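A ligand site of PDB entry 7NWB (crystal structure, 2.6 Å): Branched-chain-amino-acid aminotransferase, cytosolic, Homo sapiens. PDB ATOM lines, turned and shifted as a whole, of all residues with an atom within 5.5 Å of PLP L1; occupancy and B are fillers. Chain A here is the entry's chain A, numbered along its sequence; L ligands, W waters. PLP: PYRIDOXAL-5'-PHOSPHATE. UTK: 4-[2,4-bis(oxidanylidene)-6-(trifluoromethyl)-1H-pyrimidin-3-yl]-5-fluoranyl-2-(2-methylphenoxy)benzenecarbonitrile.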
ATOM      1  N   PHE A  98      10.134  10.862   4.416  1.00  0.00           N
ATOM      2  CA  PHE A  98      10.689   9.508   4.300  1.00  0.00           C
ATOM      3  C   PHE A  98      11.206   9.042   5.663  1.00  0.00           C
ATOM      4  O   PHE A  98      11.336   9.846   6.609  1.00  0.00           O
ATOM      5  CB  PHE A  98      11.789   9.488   3.242  1.00  0.00           C
ATOM      6  CG  PHE A  98      13.005  10.296   3.602  1.00  0.00           C
ATOM      7  CD1 PHE A  98      13.030  11.664   3.436  1.00  0.00           C
ATOM      8  CD2 PHE A  98      14.136   9.671   4.121  1.00  0.00           C
ATOM      9  CE1 PHE A  98      14.145  12.402   3.782  1.00  0.00           C
ATOM     10  CE2 PHE A  98      15.252  10.416   4.455  1.00  0.00           C
ATOM     11  CZ  PHE A  98      15.266  11.775   4.281  1.00  0.00           C
ATOM     12  N   GLY A 100      14.226   5.869   7.167  1.00  0.00           N
ATOM     13  CA  GLY A 100      15.362   4.978   6.895  1.00  0.00           C
ATOM     14  C   GLY A 100      15.576   4.076   8.094  1.00  0.00           C
ATOM     15  O   GLY A 100      15.795   4.608   9.198  1.00  0.00           O
ATOM     16  N   ASN A 119      11.126   4.707  14.384  1.00  0.00           N
ATOM     17  CA  ASN A 119      11.005   5.199  12.989  1.00  0.00           C
ATOM     18  C   ASN A 119       9.527   5.528  12.703  1.00  0.00           C
ATOM     19  O   ASN A 119       9.251   6.599  12.150  1.00  0.00           O
ATOM     20  CB  ASN A 119      11.562   4.186  11.983  1.00  0.00           C
ATOM     21  CG  ASN A 119      13.056   4.022  12.092  1.00  0.00           C
ATOM     22  OD1 ASN A 119      13.815   4.704  11.399  1.00  0.00           O
ATOM     23  ND2 ASN A 119      13.484   3.121  12.947  1.00  0.00           N
ATOM     24  N   ARG A 122       8.530   8.729  14.424  1.00  0.00           N
ATOM     25  CA  ARG A 122       9.150   9.889  13.736  1.00  0.00           C
ATOM     26  C   ARG A 122       8.427  10.163  12.411  1.00  0.00           C
ATOM     27  O   ARG A 122       8.243  11.357  12.069  1.00  0.00           O
ATOM     28  CB  ARG A 122      10.641   9.611  13.508  1.00  0.00           C
ATOM     29  CG  ARG A 122      11.465  10.859  13.223  1.00  0.00           C
ATOM     30  CD  ARG A 122      12.942  10.557  13.354  1.00  0.00           C
ATOM     31  NE  ARG A 122      13.395   9.597  12.344  1.00  0.00           N
ATOM     32  CZ  ARG A 122      14.566   8.990  12.352  1.00  0.00           C
ATOM     33  NH1 ARG A 122      15.448   9.220  13.310  1.00  0.00           N
ATOM     34  NH2 ARG A 122      14.855   8.149  11.382  1.00  0.00           N
ATOM     35  N   ARG A 215      21.510  24.418   7.671  1.00  0.00           N
ATOM     36  CA  ARG A 215      20.679  23.224   7.381  1.00  0.00           C
ATOM     37  C   ARG A 215      19.248  23.447   7.898  1.00  0.00           C
ATOM     38  O   ARG A 215      18.309  22.947   7.256  1.00  0.00           O
ATOM     39  CB  ARG A 215      21.252  21.999   8.106  1.00  0.00           C
ATOM     40  CG  ARG A 215      20.721  20.670   7.590  1.00  0.00           C
ATOM     41  CD  ARG A 215      21.089  19.536   8.534  1.00  0.00           C
ATOM     42  NE  ARG A 215      20.305  19.553   9.771  1.00  0.00           N
ATOM     43  CZ  ARG A 215      19.083  19.064   9.879  1.00  0.00           C
ATOM     44  NH1 ARG A 215      18.478  18.500   8.837  1.00  0.00           N
ATOM     45  NH2 ARG A 215      18.444  19.121  11.033  1.00  0.00           N
ATOM     46  N   GLY A 222      13.707  21.081  10.618  1.00  0.00           N
ATOM     47  CA  GLY A 222      14.998  20.362  10.728  1.00  0.00           C
ATOM     48  C   GLY A 222      14.883  19.102  11.580  1.00  0.00           C
ATOM     49  O   GLY A 222      15.672  18.168  11.341  1.00  0.00           O
ATOM     50  N   LYS A 225      12.082  14.332   9.112  1.00  0.00           N
ATOM     51  CA  LYS A 225      12.641  13.752   7.878  1.00  0.00           C
ATOM     52  C   LYS A 225      11.705  14.142   6.728  1.00  0.00           C
ATOM     53  O   LYS A 225      11.195  13.243   6.035  1.00  0.00           O
ATOM     54  CB  LYS A 225      12.899  12.244   8.032  1.00  0.00           C
ATOM     55  CG  LYS A 225      14.363  11.900   8.271  1.00  0.00           C
ATOM     56  CD  LYS A 225      14.671  10.445   8.485  1.00  0.00           C
ATOM     57  CE  LYS A 225      16.099  10.101   8.108  1.00  0.00           C
ATOM     58  NZ  LYS A 225      17.086  10.847   8.923  1.00  0.00           N
ATOM     59  N   TYR A 230      16.537  18.340   2.743  1.00  0.00           N
ATOM     60  CA  TYR A 230      17.678  17.624   2.101  1.00  0.00           C
ATOM     61  C   TYR A 230      18.046  18.298   0.769  1.00  0.00           C
ATOM     62  O   TYR A 230      19.254  18.399   0.507  1.00  0.00           O
ATOM     63  CB  TYR A 230      17.398  16.118   2.086  1.00  0.00           C
ATOM     64  CG  TYR A 230      17.156  15.622   3.487  1.00  0.00           C
ATOM     65  CD1 TYR A 230      18.207  15.315   4.347  1.00  0.00           C
ATOM     66  CD2 TYR A 230      15.879  15.631   3.999  1.00  0.00           C
ATOM     67  CE1 TYR A 230      17.979  14.947   5.657  1.00  0.00           C
ATOM     68  CE2 TYR A 230      15.632  15.266   5.320  1.00  0.00           C
ATOM     69  CZ  TYR A 230      16.688  14.934   6.152  1.00  0.00           C
ATOM     70  OH  TYR A 230      16.395  14.611   7.439  1.00  0.00           O
ATOM     71  N   GLU A 260      25.358  18.967  13.174  1.00  0.00           N
ATOM     72  CA  GLU A 260      25.208  17.655  12.487  1.00  0.00           C
ATOM     73  C   GLU A 260      26.370  17.466  11.511  1.00  0.00           C
ATOM     74  O   GLU A 260      26.893  18.473  11.003  1.00  0.00           O
ATOM     75  CB  GLU A 260      23.876  17.566  11.740  1.00  0.00           C
ATOM     76  CG  GLU A 260      22.668  17.719  12.642  1.00  0.00           C
ATOM     77  CD  GLU A 260      21.577  16.683  12.431  1.00  0.00           C
ATOM     78  OE1 GLU A 260      21.893  15.578  11.945  1.00  0.00           O
ATOM     79  OE2 GLU A 260      20.423  16.968  12.785  1.00  0.00           O
ATOM     80  N   GLY A 262      26.731  16.045   8.054  1.00  0.00           N
ATOM     81  CA  GLY A 262      25.906  15.674   6.892  1.00  0.00           C
ATOM     82  C   GLY A 262      24.515  15.297   7.325  1.00  0.00           C
ATOM     83  O   GLY A 262      23.835  16.150   7.916  1.00  0.00           O
ATOM     84  N   THR A 263      24.112  14.048   7.095  1.00  0.00           N
ATOM     85  CA  THR A 263      22.815  13.465   7.524  1.00  0.00           C
ATOM     86  C   THR A 263      23.051  12.506   8.700  1.00  0.00           C
ATOM     87  O   THR A 263      22.331  11.469   8.787  1.00  0.00           O
ATOM     88  CB  THR A 263      22.106  12.837   6.314  1.00  0.00           C
ATOM     89  OG1 THR A 263      22.950  11.850   5.716  1.00  0.00           O
ATOM     90  CG2 THR A 263      21.751  13.862   5.265  1.00  0.00           C
ATOM     91  N   MET A 264      24.025  12.841   9.557  1.00  0.00           N
ATOM     92  CA  MET A 264      24.398  12.076  10.779  1.00  0.00           C
ATOM     93  C   MET A 264      24.412  13.017  11.983  1.00  0.00           C
ATOM     94  O   MET A 264      24.834  14.183  11.830  1.00  0.00           O
ATOM     95  CB  MET A 264      25.786  11.458  10.637  1.00  0.00           C
ATOM     96  CG  MET A 264      25.906  10.345   9.614  1.00  0.00           C
ATOM     97  SD  MET A 264      27.619   9.822   9.434  1.00  0.00           S
ATOM     98  CE  MET A 264      28.174  10.975   8.193  1.00  0.00           C
ATOM     99  N   ASN A 265      23.993  12.526  13.139  1.00  0.00           N
ATOM    100  CA  ASN A 265      24.112  13.262  14.430  1.00  0.00           C
ATOM    101  C   ASN A 265      25.582  13.310  14.832  1.00  0.00           C
ATOM    102  O   ASN A 265      26.297  12.371  14.496  1.00  0.00           O
ATOM    103  CB  ASN A 265      23.268  12.622  15.515  1.00  0.00           C
ATOM    104  CG  ASN A 265      21.793  12.811  15.259  1.00  0.00           C
ATOM    105  OD1 ASN A 265      21.083  11.835  15.023  1.00  0.00           O
ATOM    106  ND2 ASN A 265      21.354  14.066  15.293  1.00  0.00           N
ATOM    107  N   LEU A 289      17.800  16.596  13.940  1.00  0.00           N
ATOM    108  CA  LEU A 289      16.978  15.392  13.652  1.00  0.00           C
ATOM    109  C   LEU A 289      17.164  14.438  14.819  1.00  0.00           C
ATOM    110  O   LEU A 289      18.291  14.053  15.109  1.00  0.00           O
ATOM    111  CB  LEU A 289      17.439  14.779  12.326  1.00  0.00           C
ATOM    112  CG  LEU A 289      16.484  13.788  11.657  1.00  0.00           C
ATOM    113  CD1 LEU A 289      16.485  12.439  12.366  1.00  0.00           C
ATOM    114  CD2 LEU A 289      15.071  14.342  11.567  1.00  0.00           C
ATOM    115  N   PRO A 290      16.103  14.058  15.571  1.00  0.00           N
ATOM    116  CA  PRO A 290      16.246  13.097  16.660  1.00  0.00           C
ATOM    117  C   PRO A 290      16.532  11.700  16.108  1.00  0.00           C
ATOM    118  O   PRO A 290      15.620  10.965  15.814  1.00  0.00           O
ATOM    119  CB  PRO A 290      14.898  13.139  17.393  1.00  0.00           C
ATOM    120  CG  PRO A 290      14.197  14.357  16.837  1.00  0.00           C
ATOM    121  CD  PRO A 290      14.729  14.529  15.431  1.00  0.00           C
ATOM    122  N   GLY A 291      17.818  11.386  15.935  1.00  0.00           N
ATOM    123  CA  GLY A 291      18.272  10.115  15.357  1.00  0.00           C
ATOM    124  C   GLY A 291      17.960   8.953  16.284  1.00  0.00           C
ATOM    125  O   GLY A 291      17.975   9.140  17.500  1.00  0.00           O
ATOM    126  N   VAL A 292      17.681   7.788  15.712  1.00  0.00           N
ATOM    127  CA  VAL A 292      17.522   6.519  16.476  1.00  0.00           C
ATOM    128  C   VAL A 292      18.889   6.139  17.059  1.00  0.00           C
ATOM    129  O   VAL A 292      18.972   5.847  18.263  1.00  0.00           O
ATOM    130  CB  VAL A 292      16.957   5.384  15.599  1.00  0.00           C
ATOM    131  CG1 VAL A 292      16.865   4.080  16.386  1.00  0.00           C
ATOM    132  CG2 VAL A 292      15.601   5.774  15.024  1.00  0.00           C
ATOM    133  N   THR A 293      19.920   6.160  16.210  1.00  0.00           N
ATOM    134  CA  THR A 293      21.295   5.794  16.628  1.00  0.00           C
ATOM    135  C   THR A 293      21.709   6.724  17.765  1.00  0.00           C
ATOM    136  O   THR A 293      22.223   6.225  18.779  1.00  0.00           O
ATOM    137  CB  THR A 293      22.252   5.782  15.433  1.00  0.00           C
ATOM    138  OG1 THR A 293      21.589   5.174  14.329  1.00  0.00           O
ATOM    139  CG2 THR A 293      23.544   5.040  15.729  1.00  0.00           C
ATOM    140  N   ARG A 294      21.423   8.024  17.624  1.00  0.00           N
ATOM    141  CA  ARG A 294      21.707   9.066  18.649  1.00  0.00           C
ATOM    142  C   ARG A 294      21.089   8.639  19.986  1.00  0.00           C
ATOM    143  O   ARG A 294      21.814   8.662  20.992  1.00  0.00           O
ATOM    144  CB  ARG A 294      21.178  10.427  18.175  1.00  0.00           C
ATOM    145  CG  ARG A 294      21.273  11.561  19.185  1.00  0.00           C
ATOM    146  CD  ARG A 294      20.632  12.847  18.657  1.00  0.00           C
ATOM    147  NE  ARG A 294      20.701  13.952  19.591  1.00  0.00           N
ATOM    148  CZ  ARG A 294      19.983  14.036  20.714  1.00  0.00           C
ATOM    149  NH1 ARG A 294      19.119  13.085  21.037  1.00  0.00           N
ATOM    150  NH2 ARG A 294      20.139  15.060  21.525  1.00  0.00           N
ATOM    151  N   SER A 334      26.815   9.694  13.851  1.00  0.00           N
ATOM    152  CA  SER A 334      25.936   8.553  14.183  1.00  0.00           C
ATOM    153  C   SER A 334      24.734   8.571  13.243  1.00  0.00           C
ATOM    154  O   SER A 334      24.286   9.676  12.895  1.00  0.00           O
ATOM    155  CB  SER A 334      25.503   8.590  15.635  1.00  0.00           C
ATOM    156  OG  SER A 334      24.326   9.347  15.797  1.00  0.00           O
ATOM    157  N   GLY A 335      24.218   7.399  12.895  1.00  0.00           N
ATOM    158  CA  GLY A 335      23.065   7.244  11.999  1.00  0.00           C
ATOM    159  C   GLY A 335      22.934   5.811  11.531  1.00  0.00           C
ATOM    160  O   GLY A 335      23.895   5.032  11.706  1.00  0.00           O
ATOM    161  N   THR A 336      21.777   5.483  10.964  1.00  0.00           N
ATOM    162  CA  THR A 336      21.435   4.138  10.432  1.00  0.00           C
ATOM    163  C   THR A 336      22.470   3.777   9.357  1.00  0.00           C
ATOM    164  O   THR A 336      22.803   2.582   9.228  1.00  0.00           O
ATOM    165  CB  THR A 336      19.976   4.115   9.935  1.00  0.00           C
ATOM    166  OG1 THR A 336      19.107   4.117  11.066  1.00  0.00           O
ATOM    167  CG2 THR A 336      19.653   2.901   9.078  1.00  0.00           C
ATOM    168  N   ALA A 337      22.946   4.774   8.619  1.00  0.00           N
ATOM    169  CA  ALA A 337      23.855   4.620   7.458  1.00  0.00           C
ATOM    170  C   ALA A 337      25.153   3.973   7.911  1.00  0.00           C
ATOM    171  O   ALA A 337      25.538   2.935   7.392  1.00  0.00           O
ATOM    172  CB  ALA A 337      24.139   5.968   6.848  1.00  0.00           C
HETATM  173  N1  PLP L   1      20.505  13.824  10.874  1.00  0.00           N
HETATM  174  C2  PLP L   1      19.674  13.994   9.843  1.00  0.00           C
HETATM  175  C2A PLP L   1      19.583  15.335   9.211  1.00  0.00           C
HETATM  176  C3  PLP L   1      18.916  12.926   9.369  1.00  0.00           C
HETATM  177  O3  PLP L   1      18.091  13.144   8.321  1.00  0.00           O
HETATM  178  C4  PLP L   1      19.025  11.652   9.991  1.00  0.00           C
HETATM  179  C4A PLP L   1      18.211  10.552   9.464  1.00  0.00           C
HETATM  180  C5  PLP L   1      19.902  11.506  11.087  1.00  0.00           C
HETATM  181  C6  PLP L   1      20.613  12.618  11.475  1.00  0.00           C
HETATM  182  C5A PLP L   1      20.142  10.212  11.817  1.00  0.00           C
HETATM  183  O4P PLP L   1      18.995   9.307  11.872  1.00  0.00           O
HETATM  184  P   PLP L   1      19.086   7.761  12.373  1.00  0.00           P
HETATM  185  O1P PLP L   1      17.654   7.446  12.839  1.00  0.00           O
HETATM  186  O2P PLP L   1      19.526   6.965  11.157  1.00  0.00           O
HETATM  187  O3P PLP L   1      20.064   7.684  13.535  1.00  0.00           O
HETATM  188  N1  UTK L   2      24.618   9.108   2.580  1.00  0.00           N
HETATM  189  C4  UTK L   2      25.751   9.537   3.254  1.00  0.00           C
HETATM  190  C5  UTK L   2      22.710   8.393   3.887  1.00  0.00           C
HETATM  191  C6  UTK L   2      24.320   6.786   2.952  1.00  0.00           C
HETATM  192  C7  UTK L   2      25.096  10.639   0.750  1.00  0.00           C
HETATM  193  C15 UTK L   2      22.477   5.955   4.222  1.00  0.00           C
HETATM  194  C17 UTK L   2      27.167  12.159   0.884  1.00  0.00           C
HETATM  195  C24 UTK L   2      19.657   8.998   3.690  1.00  0.00           C
HETATM  196  C26 UTK L   2      18.972  10.180   3.574  1.00  0.00           C
HETATM  197  C28 UTK L   2      19.363  10.628   5.919  1.00  0.00           C
HETATM  198  C27 UTK L   2      19.785   8.145   2.446  1.00  0.00           C
HETATM  199  C29 UTK L   2      18.824  10.984   4.685  1.00  0.00           C
HETATM  200  C25 UTK L   2      20.060   9.464   6.031  1.00  0.00           C
HETATM  201  C19 UTK L   2      20.207   8.651   4.922  1.00  0.00           C
HETATM  202  O16 UTK L   2      20.878   7.505   5.124  1.00  0.00           O
HETATM  203  C11 UTK L   2      22.023   7.298   4.416  1.00  0.00           C
HETATM  204  C18 UTK L   2      21.725   4.887   4.801  1.00  0.00           C
HETATM  205  N23 UTK L   2      21.109   4.036   5.250  1.00  0.00           N
HETATM  206  C12 UTK L   2      23.634   5.692   3.481  1.00  0.00           C
HETATM  207  F13 UTK L   2      25.452   6.551   2.238  1.00  0.00           F
HETATM  208  C2  UTK L   2      23.864   8.110   3.148  1.00  0.00           C
HETATM  209  C3  UTK L   2      24.294   9.649   1.329  1.00  0.00           C
HETATM  210  O8  UTK L   2      23.278   9.249   0.747  1.00  0.00           O
HETATM  211  C14 UTK L   2      26.231  11.079   1.433  1.00  0.00           C
HETATM  212  F21 UTK L   2      26.694  12.614  -0.256  1.00  0.00           F
HETATM  213  F22 UTK L   2      28.374  11.636   0.676  1.00  0.00           F
HETATM  214  F20 UTK L   2      27.281  13.164   1.731  1.00  0.00           F
HETATM  215  N9  UTK L   2      26.542  10.526   2.655  1.00  0.00           N
HETATM  216  O10 UTK L   2      26.039   9.070   4.354  1.00  0.00           O
HETATM  217  O   HOH W   1      21.705   9.120  15.068  1.00  0.00           O
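The side-chain hydroxyl (OG1) of Thr 336 is in hydrogen-bond range of an oxygen (O2P) of PLP L1, at 2.9 Å. OG1 of Thr 293 is in hydrogen-bond range of O3P of PLP L1, at 3.0 Å. An oxygen (O1P) of PLP L1 is in salt-bridge range of the guanidinium group (NH1) of Arg 122 (2.9 Å). The backbone NH of Val 292 lies within hydrogen-bond range of an oxygen (O1P) of PLP L1, 2.9 Å away. A nitrogen (N1) of PLP L1 is in hydrogen-bond range of the side-chain carboxylate of Glu 260 (2.5 Å). The backbone NH (N) of Thr 336 lies within hydrogen-bond range of an oxygen (O2P) of PLP L1, at 2.7 Å. The backbone NH of Thr 293 lies within hydrogen-bond range of an oxygen (O3P) of PLP L1 (3.1 Å). The side-chain amino group of Lys 225 is bonded to a carbon (C4A) of PLP L1 (1.3 Å). The side-chain hydroxyl (OH) of Tyr 230 sits at hydrogen-bond distance from an oxygen (O3) of PLP L1, 2.4 Å away.
The backbone NH (N) of Thr 336 is in hydrogen-bond range of the side-chain hydroxyl (OG1) of Thr 293. The side-chain hydroxyl (OG1) of Thr 293 lies close to the backbone carbonyl oxygen (O) of Gly 335, at 3.5 Å. OE2 of Glu 260 sits at hydrogen-bond distance from N of Leu 289, at 2.9 Å. The side-chain carboxylate (OE2) of Glu 260 is in salt-bridge range of the guanidinium group (NH2) of Arg 215 (3.4 Å). The backbone carbonyl oxygen of Gly 222 lies within hydrogen-bond range of the guanidinium group of Arg 215 (2.9 Å). The backbone NH of Ser 334 lies within hydrogen-bond range of the backbone carbonyl oxygen of Asn 265, at 2.8 Å. The side-chain amide nitrogen (ND2) of Asn 265 lies within hydrogen-bond range of the backbone carbonyl oxygen (O) of Leu 289 (3.1 Å). The guanidinium group (NH1) of Arg 122 sits at hydrogen-bond distance from the backbone carbonyl oxygen (O) of Pro 290 (3.1 Å).
Merely in contact with PLP L1: Arg 215 (3.4 Å), Thr 263 (3.3 Å), Met 264 (3.9 Å), Asn 265 (3.7 Å), Leu 289 (3.4 Å), Gly 291 (3.5 Å) and Gly 335 (3.4 Å). Hydrophobic or aromatic side chains that line PLP L1: Tyr 230, Leu 289 and Val 292. Of the 23 residues printed, 14 come within 4 Å of PLP L1.
Water W1 lies within hydrogen-bond range of O3P of PLP L1 (2.7 Å), OG of Ser 334 (2.7 Å), OD1 of Asn 265 (2.8 Å) and N of Arg 294 (2.8 Å).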
